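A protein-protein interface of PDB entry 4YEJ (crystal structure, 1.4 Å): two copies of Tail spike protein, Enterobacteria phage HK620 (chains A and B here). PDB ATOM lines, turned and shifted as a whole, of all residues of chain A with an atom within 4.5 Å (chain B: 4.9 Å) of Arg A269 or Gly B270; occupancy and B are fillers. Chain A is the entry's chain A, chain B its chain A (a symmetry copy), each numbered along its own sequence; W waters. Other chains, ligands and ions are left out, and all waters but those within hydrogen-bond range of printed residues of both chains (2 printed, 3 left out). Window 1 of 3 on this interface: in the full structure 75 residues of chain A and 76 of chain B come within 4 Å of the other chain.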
ATOM      1  N   VAL A 240       1.877 -30.254 -20.194  1.00  0.00           N
ATOM      2  CA  VAL A 240       1.674 -31.499 -19.410  1.00  0.00           C
ATOM      3  C   VAL A 240       3.049 -31.950 -18.971  1.00  0.00           C
ATOM      4  O   VAL A 240       3.935 -32.135 -19.846  1.00  0.00           O
ATOM      5  CB  VAL A 240       0.986 -32.576 -20.248  1.00  0.00           C
ATOM      6  CG1 VAL A 240       0.939 -33.846 -19.455  1.00  0.00           C
ATOM      7  CG2 VAL A 240      -0.394 -32.117 -20.649  1.00  0.00           C
ATOM      8  N   GLU A 241       3.273 -32.210 -17.701  1.00  0.00           N
ATOM      9  CA  GLU A 241       4.543 -32.729 -17.222  1.00  0.00           C
ATOM     10  C   GLU A 241       4.431 -33.747 -16.165  1.00  0.00           C
ATOM     11  O   GLU A 241       3.549 -33.640 -15.292  1.00  0.00           O
ATOM     12  CB  GLU A 241       5.600 -31.666 -16.873  1.00  0.00           C
ATOM     13  CG  GLU A 241       5.230 -30.520 -16.109  1.00  0.00           C
ATOM     14  CD  GLU A 241       6.328 -29.417 -15.926  1.00  0.00           C
ATOM     15  OE1 GLU A 241       7.503 -29.569 -16.299  1.00  0.00           O
ATOM     16  OE2 GLU A 241       5.935 -28.353 -15.378  1.00  0.00           O
ATOM     17  N   SER A 242       5.238 -34.797 -16.253  1.00  0.00           N
ATOM     18  CA  SER A 242       5.391 -35.764 -15.136  1.00  0.00           C
ATOM     19  C   SER A 242       4.078 -36.422 -14.804  1.00  0.00           C
ATOM     20  O   SER A 242       3.768 -36.550 -13.604  1.00  0.00           O
ATOM     21  CB  SER A 242       6.031 -35.110 -13.898  1.00  0.00           C
ATOM     22  OG  SER A 242       7.358 -34.749 -14.265  1.00  0.00           O
ATOM     23  N   PHE A 267       3.898 -27.805 -24.348  1.00  0.00           N
ATOM     24  CA  PHE A 267       4.831 -28.862 -24.070  1.00  0.00           C
ATOM     25  C   PHE A 267       4.198 -30.115 -23.488  1.00  0.00           C
ATOM     26  O   PHE A 267       3.160 -30.070 -22.774  1.00  0.00           O
ATOM     27  CB  PHE A 267       5.978 -28.388 -23.213  1.00  0.00           C
ATOM     28  CG  PHE A 267       5.557 -27.911 -21.840  1.00  0.00           C
ATOM     29  CD1 PHE A 267       5.313 -28.776 -20.797  1.00  0.00           C
ATOM     30  CD2 PHE A 267       5.383 -26.564 -21.602  1.00  0.00           C
ATOM     31  CE1 PHE A 267       4.970 -28.327 -19.493  1.00  0.00           C
ATOM     32  CE2 PHE A 267       4.977 -26.116 -20.342  1.00  0.00           C
ATOM     33  CZ  PHE A 267       4.797 -26.971 -19.301  1.00  0.00           C
ATOM     34  N   TYR A 268       4.849 -31.261 -23.692  1.00  0.00           N
ATOM     35  CA  TYR A 268       4.509 -32.562 -23.121  1.00  0.00           C
ATOM     36  C   TYR A 268       5.822 -33.226 -22.727  1.00  0.00           C
ATOM     37  O   TYR A 268       6.597 -33.625 -23.620  1.00  0.00           O
ATOM     38  CB  TYR A 268       3.696 -33.318 -24.103  1.00  0.00           C
ATOM     39  CG  TYR A 268       3.293 -34.739 -23.680  1.00  0.00           C
ATOM     40  CD1 TYR A 268       3.052 -35.051 -22.317  1.00  0.00           C
ATOM     41  CD2 TYR A 268       3.032 -35.717 -24.602  1.00  0.00           C
ATOM     42  CE1 TYR A 268       2.634 -36.329 -21.931  1.00  0.00           C
ATOM     43  CE2 TYR A 268       2.643 -36.967 -24.196  1.00  0.00           C
ATOM     44  CZ  TYR A 268       2.402 -37.250 -22.873  1.00  0.00           C
ATOM     45  OH  TYR A 268       1.971 -38.503 -22.453  1.00  0.00           O
ATOM     46  N   ARG A 269       6.128 -33.358 -21.436  1.00  0.00           N
ATOM     47  CA  ARG A 269       7.409 -33.856 -21.038  1.00  0.00           C
ATOM     48  C   ARG A 269       7.322 -34.786 -19.877  1.00  0.00           C
ATOM     49  O   ARG A 269       6.423 -34.675 -19.003  1.00  0.00           O
ATOM     50  CB  ARG A 269       8.378 -32.720 -20.692  1.00  0.00           C
ATOM     51  CG  ARG A 269       7.868 -31.959 -19.489  1.00  0.00           C
ATOM     52  CD  ARG A 269       8.683 -30.722 -19.150  1.00  0.00           C
ATOM     53  NE  ARG A 269       8.867 -29.728 -20.218  1.00  0.00           N
ATOM     54  CZ  ARG A 269       8.838 -28.394 -20.020  1.00  0.00           C
ATOM     55  NH1 ARG A 269       8.505 -27.928 -18.840  1.00  0.00           N
ATOM     56  NH2 ARG A 269       9.083 -27.498 -20.986  1.00  0.00           N
ATOM     57  N   GLY A 270       8.310 -35.669 -19.778  1.00  0.00           N
ATOM     58  CA  GLY A 270       8.528 -36.437 -18.583  1.00  0.00           C
ATOM     59  C   GLY A 270       7.440 -37.381 -18.164  1.00  0.00           C
ATOM     60  O   GLY A 270       7.343 -37.690 -16.957  1.00  0.00           O
ATOM     61  N   SER A 271       6.602 -37.831 -19.110  1.00  0.00           N
ATOM     62  CA  SER A 271       5.470 -38.629 -18.768  1.00  0.00           C
ATOM     63  C   SER A 271       5.599 -40.046 -19.247  1.00  0.00           C
ATOM     64  O   SER A 271       6.455 -40.353 -20.078  1.00  0.00           O
ATOM     65  CB  SER A 271       4.229 -37.954 -19.341  1.00  0.00           C
ATOM     66  OG  SER A 271       4.067 -36.635 -18.761  1.00  0.00           O
ATOM     67  N   GLN A 300       6.886 -28.736 -27.941  1.00  0.00           N
ATOM     68  CA  GLN A 300       7.961 -29.527 -27.338  1.00  0.00           C
ATOM     69  C   GLN A 300       7.399 -30.849 -26.842  1.00  0.00           C
ATOM     70  O   GLN A 300       6.482 -30.849 -26.019  1.00  0.00           O
ATOM     71  CB  GLN A 300       8.617 -28.739 -26.232  1.00  0.00           C
ATOM     72  CG  GLN A 300       9.733 -29.442 -25.521  1.00  0.00           C
ATOM     73  CD  GLN A 300      10.078 -28.649 -24.299  1.00  0.00           C
ATOM     74  OE1 GLN A 300       9.326 -28.647 -23.368  1.00  0.00           O
ATOM     75  NE2 GLN A 300      11.221 -28.048 -24.277  1.00  0.00           N
ATOM     76  N   GLU A 302       9.170 -33.980 -25.112  1.00  0.00           N
ATOM     77  CA  GLU A 302      10.466 -34.406 -24.640  1.00  0.00           C
ATOM     78  C   GLU A 302      10.420 -35.388 -23.490  1.00  0.00           C
ATOM     79  O   GLU A 302       9.565 -35.327 -22.602  1.00  0.00           O
ATOM     80  CB  GLU A 302      11.284 -33.164 -24.232  1.00  0.00           C
ATOM     81  CG  GLU A 302      11.891 -32.476 -25.454  1.00  0.00           C
ATOM     82  CD  GLU A 302      12.723 -31.236 -25.187  1.00  0.00           C
ATOM     83  OE1 GLU A 302      12.591 -30.653 -24.089  1.00  0.00           O
ATOM     84  OE2 GLU A 302      13.432 -30.804 -26.092  1.00  0.00           O
ATOM     85  N   ASN A 304       9.705 -38.409 -22.695  1.00  0.00           N
ATOM     86  CA  ASN A 304       8.591 -39.310 -22.354  1.00  0.00           C
ATOM     87  C   ASN A 304       8.922 -40.760 -22.574  1.00  0.00           C
ATOM     88  O   ASN A 304       9.837 -41.095 -23.347  1.00  0.00           O
ATOM     89  CB  ASN A 304       7.335 -38.954 -23.112  1.00  0.00           C
ATOM     90  CG  ASN A 304       6.971 -37.504 -22.912  1.00  0.00           C
ATOM     91  OD1 ASN A 304       6.523 -37.115 -21.827  1.00  0.00           O
ATOM     92  ND2 ASN A 304       7.038 -36.707 -23.957  1.00  0.00           N
ATOM     93  N   SER B 242      10.976 -25.220 -14.689  1.00  0.00           N
ATOM     94  CA  SER B 242       9.514 -25.196 -14.948  1.00  0.00           C
ATOM     95  C   SER B 242       8.926 -23.849 -14.620  1.00  0.00           C
ATOM     96  O   SER B 242       7.848 -23.810 -13.997  1.00  0.00           O
ATOM     97  CB  SER B 242       8.785 -26.333 -14.209  1.00  0.00           C
ATOM     98  OG  SER B 242       9.246 -27.553 -14.777  1.00  0.00           O
ATOM     99  N   CYS B 243       9.596 -22.776 -15.029  1.00  0.00           N
ATOM    100  CA  CYS B 243       9.109 -21.428 -14.810  1.00  0.00           C
ATOM    101  C   CYS B 243       8.638 -20.803 -16.119  1.00  0.00           C
ATOM    102  O   CYS B 243       8.903 -21.340 -17.254  1.00  0.00           O
ATOM    103  CB  CYS B 243      10.224 -20.541 -14.187  1.00  0.00           C
ATOM    104  SG  CYS B 243      10.505 -20.989 -12.474  1.00  0.00           S
ATOM    105  N   TYR B 268      19.172 -24.655 -15.394  1.00  0.00           N
ATOM    106  CA  TYR B 268      18.014 -23.926 -15.908  1.00  0.00           C
ATOM    107  C   TYR B 268      17.291 -24.868 -16.862  1.00  0.00           C
ATOM    108  O   TYR B 268      17.818 -25.152 -17.956  1.00  0.00           O
ATOM    109  CB  TYR B 268      18.479 -22.656 -16.515  1.00  0.00           C
ATOM    110  CG  TYR B 268      17.385 -21.786 -17.155  1.00  0.00           C
ATOM    111  CD1 TYR B 268      16.070 -21.766 -16.624  1.00  0.00           C
ATOM    112  CD2 TYR B 268      17.664 -20.911 -18.170  1.00  0.00           C
ATOM    113  CE1 TYR B 268      15.083 -20.936 -17.170  1.00  0.00           C
ATOM    114  CE2 TYR B 268      16.675 -20.124 -18.699  1.00  0.00           C
ATOM    115  CZ  TYR B 268      15.409 -20.108 -18.168  1.00  0.00           C
ATOM    116  OH  TYR B 268      14.407 -19.286 -18.672  1.00  0.00           O
ATOM    117  N   ARG B 269      16.114 -25.384 -16.506  1.00  0.00           N
ATOM    118  CA  ARG B 269      15.476 -26.371 -17.321  1.00  0.00           C
ATOM    119  C   ARG B 269      14.002 -26.166 -17.413  1.00  0.00           C
ATOM    120  O   ARG B 269      13.344 -25.643 -16.476  1.00  0.00           O
ATOM    121  CB  ARG B 269      15.747 -27.790 -16.812  1.00  0.00           C
ATOM    122  CG  ARG B 269      15.138 -27.968 -15.439  1.00  0.00           C
ATOM    123  CD  ARG B 269      15.474 -29.298 -14.782  1.00  0.00           C
ATOM    124  NE  ARG B 269      16.898 -29.638 -14.648  1.00  0.00           N
ATOM    125  CZ  ARG B 269      17.430 -30.244 -13.566  1.00  0.00           C
ATOM    126  NH1 ARG B 269      16.681 -30.441 -12.508  1.00  0.00           N
ATOM    127  NH2 ARG B 269      18.714 -30.617 -13.486  1.00  0.00           N
ATOM    128  N   GLY B 270      13.425 -26.660 -18.503  1.00  0.00           N
ATOM    129  CA  GLY B 270      11.998 -26.798 -18.614  1.00  0.00           C
ATOM    130  C   GLY B 270      11.180 -25.542 -18.565  1.00  0.00           C
ATOM    131  O   GLY B 270       9.994 -25.610 -18.178  1.00  0.00           O
ATOM    132  N   SER B 271      11.774 -24.393 -18.920  1.00  0.00           N
ATOM    133  CA  SER B 271      11.100 -23.144 -18.780  1.00  0.00           C
ATOM    134  C   SER B 271      10.760 -22.521 -20.103  1.00  0.00           C
ATOM    135  O   SER B 271      11.280 -22.930 -21.142  1.00  0.00           O
ATOM    136  CB  SER B 271      11.979 -22.227 -17.937  1.00  0.00           C
ATOM    137  OG  SER B 271      12.182 -22.802 -16.621  1.00  0.00           O
ATOM    138  N   THR B 272       9.847 -21.549 -20.108  1.00  0.00           N
ATOM    139  CA  THR B 272       9.403 -20.841 -21.279  1.00  0.00           C
ATOM    140  C   THR B 272       9.653 -19.359 -21.112  1.00  0.00           C
ATOM    141  O   THR B 272       9.278 -18.814 -20.071  1.00  0.00           O
ATOM    142  CB  THR B 272       7.928 -21.159 -21.556  1.00  0.00           C
ATOM    143  OG1 THR B 272       7.725 -22.536 -21.858  1.00  0.00           O
ATOM    144  CG2 THR B 272       7.410 -20.285 -22.776  1.00  0.00           C
ATOM    145  N   GLU B 302      18.823 -26.871 -20.195  1.00  0.00           N
ATOM    146  CA  GLU B 302      18.158 -27.921 -20.930  1.00  0.00           C
ATOM    147  C   GLU B 302      16.666 -27.726 -21.085  1.00  0.00           C
ATOM    148  O   GLU B 302      15.969 -27.223 -20.199  1.00  0.00           O
ATOM    149  CB  GLU B 302      18.437 -29.271 -20.238  1.00  0.00           C
ATOM    150  CG  GLU B 302      19.819 -29.807 -20.610  1.00  0.00           C
ATOM    151  CD  GLU B 302      20.218 -31.134 -19.993  1.00  0.00           C
ATOM    152  OE1 GLU B 302      19.593 -31.537 -18.989  1.00  0.00           O
ATOM    153  OE2 GLU B 302      21.193 -31.722 -20.454  1.00  0.00           O
ATOM    154  N   ASN B 303      16.161 -28.185 -22.215  1.00  0.00           N
ATOM    155  CA  ASN B 303      14.729 -28.374 -22.426  1.00  0.00           C
ATOM    156  C   ASN B 303      13.887 -27.120 -22.175  1.00  0.00           C
ATOM    157  O   ASN B 303      12.771 -27.222 -21.675  1.00  0.00           O
ATOM    158  CB  ASN B 303      14.200 -29.550 -21.593  1.00  0.00           C
ATOM    159  CG  ASN B 303      14.784 -30.900 -22.016  1.00  0.00           C
ATOM    160  OD1 ASN B 303      15.628 -30.987 -22.944  1.00  0.00           O
ATOM    161  ND2 ASN B 303      14.417 -31.957 -21.285  1.00  0.00           N
ATOM    162  N   ASN B 304      14.427 -25.974 -22.564  1.00  0.00           N
ATOM    163  CA  ASN B 304      13.698 -24.695 -22.508  1.00  0.00           C
ATOM    164  C   ASN B 304      13.114 -24.295 -23.834  1.00  0.00           C
ATOM    165  O   ASN B 304      13.568 -24.757 -24.896  1.00  0.00           O
ATOM    166  CB  ASN B 304      14.568 -23.581 -21.978  1.00  0.00           C
ATOM    167  CG  ASN B 304      15.170 -23.948 -20.644  1.00  0.00           C
ATOM    168  OD1 ASN B 304      14.463 -23.988 -19.630  1.00  0.00           O
ATOM    169  ND2 ASN B 304      16.475 -24.106 -20.585  1.00  0.00           N
ATOM    170  N   ILE B 305      12.141 -23.452 -23.795  1.00  0.00           N
ATOM    171  CA  ILE B 305      11.466 -22.915 -24.948  1.00  0.00           C
ATOM    172  C   ILE B 305      11.664 -21.394 -24.904  1.00  0.00           C
ATOM    173  O   ILE B 305      11.340 -20.759 -23.870  1.00  0.00           O
ATOM    174  CB  ILE B 305       9.958 -23.221 -24.900  1.00  0.00           C
ATOM    175  CG1 ILE B 305       9.694 -24.757 -24.849  1.00  0.00           C
ATOM    176  CG2 ILE B 305       9.268 -22.470 -25.994  1.00  0.00           C
ATOM    177  CD1 ILE B 305       8.224 -25.107 -24.623  1.00  0.00           C
HETATM  178  O   HOH W   1       7.173 -28.813 -12.519  1.00  0.00           O
HETATM  179  O   HOH W   2       8.084 -24.580 -19.924  1.00  0.00           O
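The side-chain amide nitrogen of Gln A300 sits at hydrogen-bond distance from the backbone carbonyl oxygen of Asn B303, at 3.1 Å. The guanidinium group of Arg A269 is in hydrogen-bond range of the backbone carbonyl oxygen of Gly B270 (2.8 Å). OE1 of Glu A302 lies close to OD1 of Asn B303. The side-chain carboxylate of Glu A241 is in hydrogen-bond range of the side-chain hydroxyl of Ser B242, at 3.1 Å.
The backbone NH (N) of Tyr A268 lies within hydrogen-bond range of the backbone carbonyl oxygen (O) of Gln A300 (2.9 Å). O of Tyr A268 lies within hydrogen-bond range of N of Glu A302, at 3.0 Å. The backbone carbonyl oxygen (O) of Glu A302 lies within hydrogen-bond range of the side-chain amide nitrogen (ND2) of Asn A304, at 3.2 Å. O of Arg A269 is in hydrogen-bond range of N of Ser A242 (3.0 Å). OE1 of Glu A241 lies within salt-bridge range of NH1 of Arg A269 (3.2 Å). The backbone NH (N) of Gly A270 sits at hydrogen-bond distance from the backbone carbonyl oxygen (O) of Glu A302, at 3.1 Å.
Asn B303 touches Arg A269 (O to NH2, 3.8 Å). Ile B305 touches Gln A300 (CG1 to NE2, 3.7 Å).
Printed residues of chain B within 4 Å of Arg A269: Gly B270 and Asn B303. Of the printed residues of chain B, Glu A302 touches Asn B303. Of the printed residues of chain A, Ile B305 touches Gln A300. Of the printed residues of chain B, Glu A241 touches Ser B242. Printed residues of chain A within 4 Å of Ser B242: Glu A241. Of the printed residues of chain A, Asn B303 touches Arg A269 (3.8 Å), Gln A300 (3.1 Å) and Glu A302 (3.0 Å). Tyr A268 touches none of the printed residues of chain B. Val A240 touches none of the printed residues of chain B. The nearest printed residue of chain A that does not touch Gly B270 is Glu A241 (5.0 Å).
Of the 11 printed residues of chain A, 4 touch a printed residue of chain B. Printed residues of chain B that touch a printed residue of chain A: Ser B242, Gly B270, Asn B303 and Ile B305. Hydrophobic or aromatic side chains of chain B that line the printed part of chain A: Ile B305. Along chain B the printed residues that touch a printed residue of chain A span positions 242 to 305. Among the printed residues, no Asp or Glu carboxylate lies within 4 Å of a Lys or Arg side-chain nitrogen of the other chain.
Arg A269 touches Gly B270, but with the chains exchanged Gly A270 does not touch Arg B269 (10.7 Å). Positions printed for both chains: 242, 268, 269, 270, 271, 302 and 304. Of the 6 pairs that touch across the chains among the printed residues, none has its exchanged pair printed and touching as well.
Water W2 lies within hydrogen-bond range of O of Gly B270 (2.8 Å), OG1 of Thr B272 (2.8 Å) and NH2 of Arg A269 (3.3 Å). Water W1 bridges the side-chain carboxylate (OE2) of Glu A241 (3.1 Å) and the side-chain hydroxyl (OG) of Ser B242 (3.3 Å).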
